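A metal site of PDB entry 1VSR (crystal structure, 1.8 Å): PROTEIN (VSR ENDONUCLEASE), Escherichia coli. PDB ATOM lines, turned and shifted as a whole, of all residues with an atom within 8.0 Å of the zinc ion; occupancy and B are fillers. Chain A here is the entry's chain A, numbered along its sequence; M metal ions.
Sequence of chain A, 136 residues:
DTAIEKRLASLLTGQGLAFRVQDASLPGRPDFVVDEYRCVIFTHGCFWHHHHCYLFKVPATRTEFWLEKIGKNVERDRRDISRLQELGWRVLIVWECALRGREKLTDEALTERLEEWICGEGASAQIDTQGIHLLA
The zinc ion is bound by ND1 of His 51 (2.2 Å), SG of Cys 46 (2.3 Å), SG of Cys 53 (2.3 Å) and SG of Cys 97 (2.4 Å). The zinc ion has four donor atoms within binding distance.
Of the 20 residues printed, 4 come within 4 Å of the zinc ion. The nearest printed residue that does not touch the zinc ion is Trp 95 (4.2 Å).
The side-chain carboxylate (OE1) of Glu 96 is in hydrogen-bond range of the backbone NH (N) of Cys 46 (2.9 Å). SG of Cys 53 lies close to N of Leu 55, 3.4 Å away.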
ATOM      1  N   HIS A  44     -27.316   5.485 -26.893  1.00  0.00           N
ATOM      2  CA  HIS A  44     -28.314   6.362 -27.485  1.00  0.00           C
ATOM      3  C   HIS A  44     -27.759   7.256 -28.602  1.00  0.00           C
ATOM      4  O   HIS A  44     -26.696   7.839 -28.377  1.00  0.00           O
ATOM      5  CB  HIS A  44     -28.787   7.297 -26.350  1.00  0.00           C
ATOM      6  CG  HIS A  44     -29.855   6.759 -25.444  1.00  0.00           C
ATOM      7  ND1 HIS A  44     -30.526   5.598 -25.775  1.00  0.00           N
ATOM      8  CD2 HIS A  44     -30.357   7.181 -24.252  1.00  0.00           C
ATOM      9  CE1 HIS A  44     -31.439   5.337 -24.834  1.00  0.00           C
ATOM     10  NE2 HIS A  44     -31.322   6.265 -23.912  1.00  0.00           N
ATOM     11  N   GLY A  45     -28.564   7.408 -29.657  1.00  0.00           N
ATOM     12  CA  GLY A  45     -28.191   8.345 -30.720  1.00  0.00           C
ATOM     13  C   GLY A  45     -28.352   9.757 -30.145  1.00  0.00           C
ATOM     14  O   GLY A  45     -29.311  10.009 -29.430  1.00  0.00           O
ATOM     15  N   CYS A  46     -27.506  10.693 -30.569  1.00  0.00           N
ATOM     16  CA  CYS A  46     -27.503  12.024 -29.961  1.00  0.00           C
ATOM     17  C   CYS A  46     -28.636  12.901 -30.511  1.00  0.00           C
ATOM     18  O   CYS A  46     -29.184  13.695 -29.748  1.00  0.00           O
ATOM     19  CB  CYS A  46     -26.127  12.668 -30.165  1.00  0.00           C
ATOM     20  SG  CYS A  46     -24.912  11.878 -29.061  1.00  0.00           S
ATOM     21  N   PHE A  47     -29.018  12.658 -31.769  1.00  0.00           N
ATOM     22  CA  PHE A  47     -30.176  13.393 -32.293  1.00  0.00           C
ATOM     23  C   PHE A  47     -31.467  12.920 -31.638  1.00  0.00           C
ATOM     24  O   PHE A  47     -32.256  13.697 -31.085  1.00  0.00           O
ATOM     25  CB  PHE A  47     -30.264  13.210 -33.822  1.00  0.00           C
ATOM     26  CG  PHE A  47     -31.520  13.734 -34.449  1.00  0.00           C
ATOM     27  CD1 PHE A  47     -31.754  15.104 -34.489  1.00  0.00           C
ATOM     28  CD2 PHE A  47     -32.452  12.883 -35.032  1.00  0.00           C
ATOM     29  CE1 PHE A  47     -32.919  15.606 -35.039  1.00  0.00           C
ATOM     30  CE2 PHE A  47     -33.614  13.362 -35.635  1.00  0.00           C
ATOM     31  CZ  PHE A  47     -33.819  14.726 -35.608  1.00  0.00           C
ATOM     32  N   HIS A  50     -31.855  13.667 -27.872  1.00  0.00           N
ATOM     33  CA  HIS A  50     -31.658  15.060 -27.499  1.00  0.00           C
ATOM     34  C   HIS A  50     -30.439  15.351 -26.645  1.00  0.00           C
ATOM     35  O   HIS A  50     -30.521  15.930 -25.549  1.00  0.00           O
ATOM     36  CB  HIS A  50     -32.925  15.562 -26.780  1.00  0.00           C
ATOM     37  CG  HIS A  50     -33.035  17.066 -26.745  1.00  0.00           C
ATOM     38  ND1 HIS A  50     -33.359  17.771 -25.598  1.00  0.00           N
ATOM     39  CD2 HIS A  50     -32.767  17.997 -27.676  1.00  0.00           C
ATOM     40  CE1 HIS A  50     -33.343  19.074 -25.866  1.00  0.00           C
ATOM     41  NE2 HIS A  50     -32.999  19.246 -27.127  1.00  0.00           N
ATOM     42  N   HIS A  51     -29.258  14.935 -27.117  1.00  0.00           N
ATOM     43  CA  HIS A  51     -28.048  15.217 -26.348  1.00  0.00           C
ATOM     44  C   HIS A  51     -27.696  16.680 -26.581  1.00  0.00           C
ATOM     45  O   HIS A  51     -28.198  17.364 -27.487  1.00  0.00           O
ATOM     46  CB  HIS A  51     -26.880  14.318 -26.756  1.00  0.00           C
ATOM     47  CG  HIS A  51     -25.838  14.183 -25.683  1.00  0.00           C
ATOM     48  ND1 HIS A  51     -24.509  13.981 -25.985  1.00  0.00           N
ATOM     49  CD2 HIS A  51     -25.914  14.198 -24.338  1.00  0.00           C
ATOM     50  CE1 HIS A  51     -23.826  13.857 -24.845  1.00  0.00           C
ATOM     51  NE2 HIS A  51     -24.665  13.992 -23.837  1.00  0.00           N
ATOM     52  N   HIS A  52     -26.781  17.197 -25.754  1.00  0.00           N
ATOM     53  CA  HIS A  52     -26.387  18.599 -25.832  1.00  0.00           C
ATOM     54  C   HIS A  52     -25.145  18.878 -26.663  1.00  0.00           C
ATOM     55  O   HIS A  52     -24.634  19.997 -26.631  1.00  0.00           O
ATOM     56  CB  HIS A  52     -26.138  19.087 -24.403  1.00  0.00           C
ATOM     57  CG  HIS A  52     -25.201  18.283 -23.550  1.00  0.00           C
ATOM     58  ND1 HIS A  52     -25.624  17.497 -22.513  1.00  0.00           N
ATOM     59  CD2 HIS A  52     -23.859  18.133 -23.586  1.00  0.00           C
ATOM     60  CE1 HIS A  52     -24.586  16.921 -21.916  1.00  0.00           C
ATOM     61  NE2 HIS A  52     -23.492  17.287 -22.561  1.00  0.00           N
ATOM     62  N   CYS A  53     -24.647  17.888 -27.396  1.00  0.00           N
ATOM     63  CA  CYS A  53     -23.377  18.001 -28.083  1.00  0.00           C
ATOM     64  C   CYS A  53     -23.504  18.516 -29.514  1.00  0.00           C
ATOM     65  O   CYS A  53     -24.595  18.701 -30.051  1.00  0.00           O
ATOM     66  CB  CYS A  53     -22.760  16.586 -28.113  1.00  0.00           C
ATOM     67  SG  CYS A  53     -23.758  15.467 -29.119  1.00  0.00           S
ATOM     68  N   TYR A  54     -22.357  18.543 -30.199  1.00  0.00           N
ATOM     69  CA  TYR A  54     -22.314  18.947 -31.602  1.00  0.00           C
ATOM     70  C   TYR A  54     -23.080  18.071 -32.589  1.00  0.00           C
ATOM     71  O   TYR A  54     -23.420  18.544 -33.678  1.00  0.00           O
ATOM     72  CB  TYR A  54     -20.849  19.071 -32.033  1.00  0.00           C
ATOM     73  CG  TYR A  54     -20.161  17.759 -32.374  1.00  0.00           C
ATOM     74  CD1 TYR A  54     -19.610  16.958 -31.381  1.00  0.00           C
ATOM     75  CD2 TYR A  54     -20.069  17.359 -33.705  1.00  0.00           C
ATOM     76  CE1 TYR A  54     -18.983  15.763 -31.702  1.00  0.00           C
ATOM     77  CE2 TYR A  54     -19.446  16.161 -34.034  1.00  0.00           C
ATOM     78  CZ  TYR A  54     -18.898  15.381 -33.034  1.00  0.00           C
ATOM     79  OH  TYR A  54     -18.271  14.205 -33.382  1.00  0.00           O
ATOM     80  N   LEU A  55     -23.441  16.840 -32.253  1.00  0.00           N
ATOM     81  CA  LEU A  55     -24.225  16.015 -33.154  1.00  0.00           C
ATOM     82  C   LEU A  55     -25.703  16.419 -33.174  1.00  0.00           C
ATOM     83  O   LEU A  55     -26.431  15.926 -34.041  1.00  0.00           O
ATOM     84  CB  LEU A  55     -24.103  14.525 -32.800  1.00  0.00           C
ATOM     85  CG  LEU A  55     -22.721  13.923 -33.058  1.00  0.00           C
ATOM     86  CD1 LEU A  55     -22.676  12.509 -32.493  1.00  0.00           C
ATOM     87  CD2 LEU A  55     -22.459  13.937 -34.568  1.00  0.00           C
ATOM     88  N   PHE A  56     -26.139  17.187 -32.174  1.00  0.00           N
ATOM     89  CA  PHE A  56     -27.548  17.567 -32.198  1.00  0.00           C
ATOM     90  C   PHE A  56     -27.784  18.712 -33.171  1.00  0.00           C
ATOM     91  O   PHE A  56     -27.202  19.773 -32.976  1.00  0.00           O
ATOM     92  CB  PHE A  56     -28.100  18.019 -30.842  1.00  0.00           C
ATOM     93  CG  PHE A  56     -29.595  18.127 -30.948  1.00  0.00           C
ATOM     94  CD1 PHE A  56     -30.415  17.011 -30.854  1.00  0.00           C
ATOM     95  CD2 PHE A  56     -30.196  19.361 -31.164  1.00  0.00           C
ATOM     96  CE1 PHE A  56     -31.783  17.110 -30.940  1.00  0.00           C
ATOM     97  CE2 PHE A  56     -31.568  19.479 -31.263  1.00  0.00           C
ATOM     98  CZ  PHE A  56     -32.351  18.358 -31.152  1.00  0.00           C
ATOM     99  N   VAL A  94     -24.211   5.330 -22.886  1.00  0.00           N
ATOM    100  CA  VAL A  94     -23.008   5.695 -23.618  1.00  0.00           C
ATOM    101  C   VAL A  94     -23.562   6.450 -24.836  1.00  0.00           C
ATOM    102  O   VAL A  94     -24.221   5.878 -25.704  1.00  0.00           O
ATOM    103  CB  VAL A  94     -22.194   4.465 -24.064  1.00  0.00           C
ATOM    104  CG1 VAL A  94     -20.965   4.985 -24.770  1.00  0.00           C
ATOM    105  CG2 VAL A  94     -21.862   3.569 -22.861  1.00  0.00           C
ATOM    106  N   TRP A  95     -23.320   7.754 -24.884  1.00  0.00           N
ATOM    107  CA  TRP A  95     -23.827   8.568 -25.981  1.00  0.00           C
ATOM    108  C   TRP A  95     -23.034   8.322 -27.268  1.00  0.00           C
ATOM    109  O   TRP A  95     -21.850   8.007 -27.289  1.00  0.00           O
ATOM    110  CB  TRP A  95     -23.678  10.032 -25.535  1.00  0.00           C
ATOM    111  CG  TRP A  95     -24.656  10.383 -24.449  1.00  0.00           C
ATOM    112  CD1 TRP A  95     -24.425  10.509 -23.111  1.00  0.00           C
ATOM    113  CD2 TRP A  95     -26.040  10.685 -24.693  1.00  0.00           C
ATOM    114  NE1 TRP A  95     -25.613  10.864 -22.505  1.00  0.00           N
ATOM    115  CE2 TRP A  95     -26.613  10.970 -23.443  1.00  0.00           C
ATOM    116  CE3 TRP A  95     -26.851  10.720 -25.840  1.00  0.00           C
ATOM    117  CZ2 TRP A  95     -27.954  11.321 -23.310  1.00  0.00           C
ATOM    118  CZ3 TRP A  95     -28.189  11.061 -25.729  1.00  0.00           C
ATOM    119  CH2 TRP A  95     -28.721  11.310 -24.455  1.00  0.00           C
ATOM    120  N   GLU A  96     -23.688   8.525 -28.409  1.00  0.00           N
ATOM    121  CA  GLU A  96     -23.112   8.259 -29.723  1.00  0.00           C
ATOM    122  C   GLU A  96     -21.837   9.040 -30.005  1.00  0.00           C
ATOM    123  O   GLU A  96     -20.870   8.546 -30.582  1.00  0.00           O
ATOM    124  CB  GLU A  96     -24.196   8.574 -30.766  1.00  0.00           C
ATOM    125  CG  GLU A  96     -23.722   8.499 -32.206  1.00  0.00           C
ATOM    126  CD  GLU A  96     -24.773   9.051 -33.155  1.00  0.00           C
ATOM    127  OE1 GLU A  96     -25.769   9.667 -32.711  1.00  0.00           O
ATOM    128  OE2 GLU A  96     -24.579   8.941 -34.384  1.00  0.00           O
ATOM    129  N   CYS A  97     -21.772  10.253 -29.476  1.00  0.00           N
ATOM    130  CA  CYS A  97     -20.637  11.165 -29.634  1.00  0.00           C
ATOM    131  C   CYS A  97     -19.381  10.576 -28.990  1.00  0.00           C
ATOM    132  O   CYS A  97     -18.285  10.898 -29.454  1.00  0.00           O
ATOM    133  CB  CYS A  97     -20.940  12.567 -29.102  1.00  0.00           C
ATOM    134  SG  CYS A  97     -21.558  12.713 -27.417  1.00  0.00           S
ATOM    135  N   ALA A  98     -19.501   9.668 -28.022  1.00  0.00           N
ATOM    136  CA  ALA A  98     -18.365   9.004 -27.404  1.00  0.00           C
ATOM    137  C   ALA A  98     -17.920   7.812 -28.241  1.00  0.00           C
ATOM    138  O   ALA A  98     -16.814   7.272 -28.131  1.00  0.00           O
ATOM    139  CB  ALA A  98     -18.736   8.522 -26.004  1.00  0.00           C
ATOM    140  N   LEU A  99     -18.835   7.274 -29.040  1.00  0.00           N
ATOM    141  CA  LEU A  99     -18.573   6.039 -29.778  1.00  0.00           C
ATOM    142  C   LEU A  99     -18.161   6.253 -31.230  1.00  0.00           C
ATOM    143  O   LEU A  99     -17.455   5.386 -31.754  1.00  0.00           O
ATOM    144  CB  LEU A  99     -19.837   5.171 -29.809  1.00  0.00           C
ATOM    145  CG  LEU A  99     -20.222   4.572 -28.452  1.00  0.00           C
ATOM    146  CD1 LEU A  99     -21.692   4.171 -28.471  1.00  0.00           C
ATOM    147  CD2 LEU A  99     -19.266   3.443 -28.127  1.00  0.00           C
ATOM    148  N   ILE A 127     -21.753   8.415 -20.235  1.00  0.00           N
ATOM    149  CA  ILE A 127     -20.433   8.710 -20.777  1.00  0.00           C
ATOM    150  C   ILE A 127     -20.539   9.548 -22.051  1.00  0.00           C
ATOM    151  O   ILE A 127     -21.278   9.157 -22.973  1.00  0.00           O
ATOM    152  CB  ILE A 127     -19.681   7.405 -21.106  1.00  0.00           C
ATOM    153  CG1 ILE A 127     -19.345   6.669 -19.787  1.00  0.00           C
ATOM    154  CG2 ILE A 127     -18.388   7.767 -21.812  1.00  0.00           C
ATOM    155  CD1 ILE A 127     -18.858   5.243 -20.002  1.00  0.00           C
ATOM    156  N   ASP A 128     -19.837  10.668 -22.135  1.00  0.00           N
ATOM    157  CA  ASP A 128     -19.796  11.418 -23.388  1.00  0.00           C
ATOM    158  C   ASP A 128     -18.360  11.773 -23.751  1.00  0.00           C
ATOM    159  O   ASP A 128     -17.490  11.111 -23.187  1.00  0.00           O
ATOM    160  CB  ASP A 128     -20.655  12.675 -23.315  1.00  0.00           C
ATOM    161  CG  ASP A 128     -20.258  13.594 -22.173  1.00  0.00           C
ATOM    162  OD1 ASP A 128     -19.104  13.609 -21.683  1.00  0.00           O
ATOM    163  OD2 ASP A 128     -21.217  14.320 -21.821  1.00  0.00           O
ATOM    164  N   THR A 129     -18.124  12.736 -24.630  1.00  0.00           N
ATOM    165  CA  THR A 129     -16.754  13.038 -25.038  1.00  0.00           C
ATOM    166  C   THR A 129     -15.924  13.633 -23.906  1.00  0.00           C
ATOM    167  O   THR A 129     -14.704  13.687 -24.051  1.00  0.00           O
ATOM    168  CB  THR A 129     -16.710  13.977 -26.263  1.00  0.00           C
ATOM    169  OG1 THR A 129     -17.449  15.185 -26.018  1.00  0.00           O
ATOM    170  CG2 THR A 129     -17.338  13.301 -27.483  1.00  0.00           C
HETATM  171 ZN    ZN M   1     -23.712  13.483 -27.961  1.00  0.00          ZN
